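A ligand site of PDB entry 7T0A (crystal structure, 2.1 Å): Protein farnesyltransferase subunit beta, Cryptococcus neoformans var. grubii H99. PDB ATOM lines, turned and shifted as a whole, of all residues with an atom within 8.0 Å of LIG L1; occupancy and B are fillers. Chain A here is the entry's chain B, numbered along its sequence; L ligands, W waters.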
ATOM      1  N   LEU A  50       0.330   7.615   1.274  1.00  0.00           N
ATOM      2  CA  LEU A  50       0.840   9.005   1.114  1.00  0.00           C
ATOM      3  C   LEU A  50       1.596   9.130  -0.219  1.00  0.00           C
ATOM      4  O   LEU A  50       1.549  10.206  -0.804  1.00  0.00           O
ATOM      5  CB  LEU A  50       1.687   9.331   2.335  1.00  0.00           C
ATOM      6  CG  LEU A  50       1.553   8.347   3.500  1.00  0.00           C
ATOM      7  CD1 LEU A  50       2.894   8.082   4.142  1.00  0.00           C
ATOM      8  CD2 LEU A  50       0.554   8.817   4.548  1.00  0.00           C
ATOM      9  N   SER A  52       2.015   6.785  -3.843  1.00  0.00           N
ATOM     10  CA  SER A  52       1.595   5.560  -4.566  1.00  0.00           C
ATOM     11  C   SER A  52       2.791   4.646  -4.904  1.00  0.00           C
ATOM     12  O   SER A  52       3.821   5.139  -5.350  1.00  0.00           O
ATOM     13  CB  SER A  52       0.789   5.922  -5.750  1.00  0.00           C
ATOM     14  OG  SER A  52       1.580   6.677  -6.625  1.00  0.00           O
ATOM     15  N   TYR A  58      -2.441   2.918 -10.282  1.00  0.00           N
ATOM     16  CA  TYR A  58      -2.936   4.021  -9.464  1.00  0.00           C
ATOM     17  C   TYR A  58      -4.455   4.047  -9.528  1.00  0.00           C
ATOM     18  O   TYR A  58      -5.040   3.971 -10.617  1.00  0.00           O
ATOM     19  CB  TYR A  58      -2.346   5.351  -9.939  1.00  0.00           C
ATOM     20  CG  TYR A  58      -2.820   6.532  -9.136  1.00  0.00           C
ATOM     21  CD1 TYR A  58      -3.552   7.556  -9.728  1.00  0.00           C
ATOM     22  CD2 TYR A  58      -2.544   6.638  -7.772  1.00  0.00           C
ATOM     23  CE1 TYR A  58      -3.989   8.647  -9.003  1.00  0.00           C
ATOM     24  CE2 TYR A  58      -2.977   7.726  -7.039  1.00  0.00           C
ATOM     25  CZ  TYR A  58      -3.697   8.721  -7.660  1.00  0.00           C
ATOM     26  OH  TYR A  58      -4.136   9.802  -6.927  1.00  0.00           O
ATOM     27  N   GLY A  60      -6.619   6.441  -8.625  1.00  0.00           N
ATOM     28  CA  GLY A  60      -7.300   7.721  -8.642  1.00  0.00           C
ATOM     29  C   GLY A  60      -8.473   7.724  -9.603  1.00  0.00           C
ATOM     30  O   GLY A  60      -8.442   7.089 -10.655  1.00  0.00           O
ATOM     31  N   LEU A  61      -9.527   8.444  -9.224  1.00  0.00           N
ATOM     32  CA  LEU A  61     -10.741   8.505 -10.035  1.00  0.00           C
ATOM     33  C   LEU A  61     -10.431   9.193 -11.359  1.00  0.00           C
ATOM     34  O   LEU A  61     -10.116  10.381 -11.394  1.00  0.00           O
ATOM     35  CB  LEU A  61     -11.844   9.230  -9.284  1.00  0.00           C
ATOM     36  CG  LEU A  61     -13.215   9.264  -9.967  1.00  0.00           C
ATOM     37  CD1 LEU A  61     -13.772   7.846 -10.103  1.00  0.00           C
ATOM     38  CD2 LEU A  61     -14.177  10.149  -9.200  1.00  0.00           C
ATOM     39  N   ILE A 486     -12.851  11.359   1.959  1.00  0.00           N
ATOM     40  CA  ILE A 486     -12.451  11.253   0.561  1.00  0.00           C
ATOM     41  C   ILE A 486     -11.248  10.320   0.498  1.00  0.00           C
ATOM     42  O   ILE A 486     -10.099  10.740   0.711  1.00  0.00           O
ATOM     43  CB  ILE A 486     -12.131  12.624  -0.058  1.00  0.00           C
ATOM     44  CG1 ILE A 486     -13.242  13.622   0.270  1.00  0.00           C
ATOM     45  CG2 ILE A 486     -11.999  12.490  -1.557  1.00  0.00           C
ATOM     46  CD1 ILE A 486     -14.571  13.279  -0.357  1.00  0.00           C
ATOM     47  N   VAL A 487     -11.503   9.049   0.208  1.00  0.00           N
ATOM     48  CA  VAL A 487     -10.433   8.060   0.106  1.00  0.00           C
ATOM     49  C   VAL A 487      -9.558   8.379  -1.103  1.00  0.00           C
ATOM     50  O   VAL A 487     -10.067   8.637  -2.205  1.00  0.00           O
ATOM     51  CB  VAL A 487     -11.014   6.643   0.019  1.00  0.00           C
ATOM     52  CG1 VAL A 487      -9.909   5.619  -0.209  1.00  0.00           C
ATOM     53  CG2 VAL A 487     -11.797   6.307   1.270  1.00  0.00           C
ATOM     54  N   GLY A 488      -8.240   8.387  -0.900  1.00  0.00           N
ATOM     55  CA  GLY A 488      -7.297   8.566  -1.985  1.00  0.00           C
ATOM     56  C   GLY A 488      -6.895   9.994  -2.266  1.00  0.00           C
ATOM     57  O   GLY A 488      -6.107  10.219  -3.195  1.00  0.00           O
ATOM     58  N   GLY A 489      -7.394  10.965  -1.522  1.00  0.00           N
ATOM     59  CA  GLY A 489      -7.054  12.347  -1.742  1.00  0.00           C
ATOM     60  C   GLY A 489      -8.233  13.145  -2.279  1.00  0.00           C
ATOM     61  O   GLY A 489      -9.168  12.621  -2.893  1.00  0.00           O
ATOM     62  N   LYS A 490      -8.166  14.468  -2.063  1.00  0.00           N
ATOM     63  CA  LYS A 490      -9.279  15.351  -2.387  1.00  0.00           C
ATOM     64  C   LYS A 490      -9.561  15.435  -3.887  1.00  0.00           C
ATOM     65  O   LYS A 490     -10.639  15.877  -4.272  1.00  0.00           O
ATOM     66  CB  LYS A 490      -9.017  16.746  -1.825  1.00  0.00           C
ATOM     67  CG  LYS A 490      -8.977  16.794  -0.305  1.00  0.00           C
ATOM     68  CD  LYS A 490      -8.748  18.202   0.207  1.00  0.00           C
ATOM     69  CE  LYS A 490      -8.675  18.231   1.727  1.00  0.00           C
ATOM     70  NZ  LYS A 490      -8.381  19.602   2.239  1.00  0.00           N
ATOM     71  N   ASP A 491      -8.617  15.015  -4.734  1.00  0.00           N
ATOM     72  CA  ASP A 491      -8.885  14.978  -6.170  1.00  0.00           C
ATOM     73  C   ASP A 491      -9.903  13.896  -6.533  1.00  0.00           C
ATOM     74  O   ASP A 491     -10.440  13.926  -7.640  1.00  0.00           O
ATOM     75  CB  ASP A 491      -7.589  14.766  -6.946  1.00  0.00           C
ATOM     76  CG  ASP A 491      -6.731  16.016  -7.006  1.00  0.00           C
ATOM     77  OD1 ASP A 491      -7.297  17.119  -7.198  1.00  0.00           O
ATOM     78  OD2 ASP A 491      -5.502  15.907  -6.852  1.00  0.00           O
ATOM     79  N   ASN A 492     -10.161  12.949  -5.636  1.00  0.00           N
ATOM     80  CA  ASN A 492     -11.202  11.950  -5.859  1.00  0.00           C
ATOM     81  C   ASN A 492     -12.584  12.433  -5.455  1.00  0.00           C
ATOM     82  O   ASN A 492     -13.565  11.714  -5.682  1.00  0.00           O
ATOM     83  CB  ASN A 492     -10.880  10.660  -5.106  1.00  0.00           C
ATOM     84  CG  ASN A 492      -9.733   9.877  -5.724  1.00  0.00           C
ATOM     85  OD1 ASN A 492      -9.434  10.038  -6.906  1.00  0.00           O
ATOM     86  ND2 ASN A 492      -9.111   9.014  -4.930  1.00  0.00           N
ATOM     87  N   ARG A 493     -12.682  13.624  -4.864  1.00  0.00           N
ATOM     88  CA  ARG A 493     -13.966  14.116  -4.386  1.00  0.00           C
ATOM     89  C   ARG A 493     -14.901  14.382  -5.555  1.00  0.00           C
ATOM     90  O   ARG A 493     -14.509  14.997  -6.556  1.00  0.00           O
ATOM     91  CB  ARG A 493     -13.786  15.395  -3.568  1.00  0.00           C
ATOM     92  CG  ARG A 493     -15.087  15.955  -3.020  1.00  0.00           C
ATOM     93  CD  ARG A 493     -14.996  17.445  -2.750  1.00  0.00           C
ATOM     94  NE  ARG A 493     -16.265  17.971  -2.220  1.00  0.00           N
ATOM     95  CZ  ARG A 493     -17.267  18.394  -2.971  1.00  0.00           C
ATOM     96  NH1 ARG A 493     -17.177  18.365  -4.300  1.00  0.00           N
ATOM     97  NH2 ARG A 493     -18.373  18.860  -2.405  1.00  0.00           N
HETATM   98  O1  LIG L   1      -4.219  16.780   0.226  1.00  0.00           O
HETATM   99  O2  LIG L   1      -5.938  15.206  -0.654  1.00  0.00           O
HETATM  100  O3  LIG L   1      -5.479  15.580  -3.676  1.00  0.00           O
HETATM  101  O4  LIG L   1      -5.486  17.459  -1.610  1.00  0.00           O
HETATM  102  C1  LIG L   1      -1.845  13.658  -9.286  1.00  0.00           C
HETATM  103  C2  LIG L   1      -1.098  14.241  -8.079  1.00  0.00           C
HETATM  104  C3  LIG L   1      -2.869  12.602  -8.863  1.00  0.00           C
HETATM  105  C4  LIG L   1      -2.057  14.758  -7.008  1.00  0.00           C
HETATM  106  C5  LIG L   1      -3.832  13.124  -7.800  1.00  0.00           C
HETATM  107  C6  LIG L   1      -3.518  14.369  -4.352  1.00  0.00           C
HETATM  108  C7  LIG L   1      -3.641  15.475  -2.117  1.00  0.00           C
HETATM  109  N1  LIG L   1      -4.056  14.344  -5.694  1.00  0.00           N
HETATM  110  C8  LIG L   1      -4.076  15.560  -3.575  1.00  0.00           C
HETATM  111  C9  LIG L   1      -3.095  13.715  -6.597  1.00  0.00           C
HETATM  112  S1  LIG L   1      -4.872  16.213  -1.011  1.00  0.00           S
HETATM  113  O1  LG2 L   2      -7.283   9.540 -15.849  1.00  0.00           O
HETATM  114  O2  LG2 L   2      -9.363  10.819 -16.369  1.00  0.00           O
HETATM  115  O3  LG2 L   2      -5.126  10.983 -16.859  1.00  0.00           O
HETATM  116  O4  LG2 L   2      -7.348  11.804 -15.289  1.00  0.00           O
HETATM  117  C1  LG2 L   2      -0.494  14.037 -20.592  1.00  0.00           C
HETATM  118  C2  LG2 L   2      -0.834  12.683 -21.228  1.00  0.00           C
HETATM  119  C3  LG2 L   2      -1.753  14.774 -20.114  1.00  0.00           C
HETATM  120  C4  LG2 L   2      -1.698  11.821 -20.323  1.00  0.00           C
HETATM  121  C5  LG2 L   2      -2.614  13.909 -19.199  1.00  0.00           C
HETATM  122  C6  LG2 L   2      -5.047  11.666 -19.150  1.00  0.00           C
HETATM  123  C7  LG2 L   2      -7.219  11.251 -17.999  1.00  0.00           C
HETATM  124  N1  LG2 L   2      -3.631  11.729 -18.832  1.00  0.00           N
HETATM  125  C8  LG2 L   2      -5.751  10.815 -18.107  1.00  0.00           C
HETATM  126  C9  LG2 L   2      -2.953  12.555 -19.836  1.00  0.00           C
HETATM  127  S1  LG2 L   2      -7.855  10.843 -16.340  1.00  0.00           S
HETATM  128  O   HOH W   1      -6.200  12.438  -5.136  1.00  0.00           O
HETATM  129  O   HOH W   2      -2.934  11.372  -3.278  1.00  0.00           O
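Water W1 bridges a nitrogen (N1) of LIG L1 (2.9 Å) and the backbone carbonyl oxygen of Gly 488 (2.9 Å).
Tyr 58 touches LIG L1 (OH to C5, 3.4 Å).
CA of Gly 489 touches O2 of LIG L1, at 3.3 Å.
Of the 13 residues printed, 4 come within 4 Å of LIG L1.
The nearest printed residue that does not touch LIG L1 is Gly 488 (5.0 Å).
The backbone NH (N) of Lys 490 is in hydrogen-bond range of an oxygen (O2) of LIG L1 (2.7 Å).
The side-chain carboxylate (OD2) of Asp 491 lies within salt-bridge range of a nitrogen (N1) of LIG L1 (2.4 Å).
An oxygen (O3) of LIG L1 is in hydrogen-bond range of the backbone NH (N) of Asp 491 (3.4 Å).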
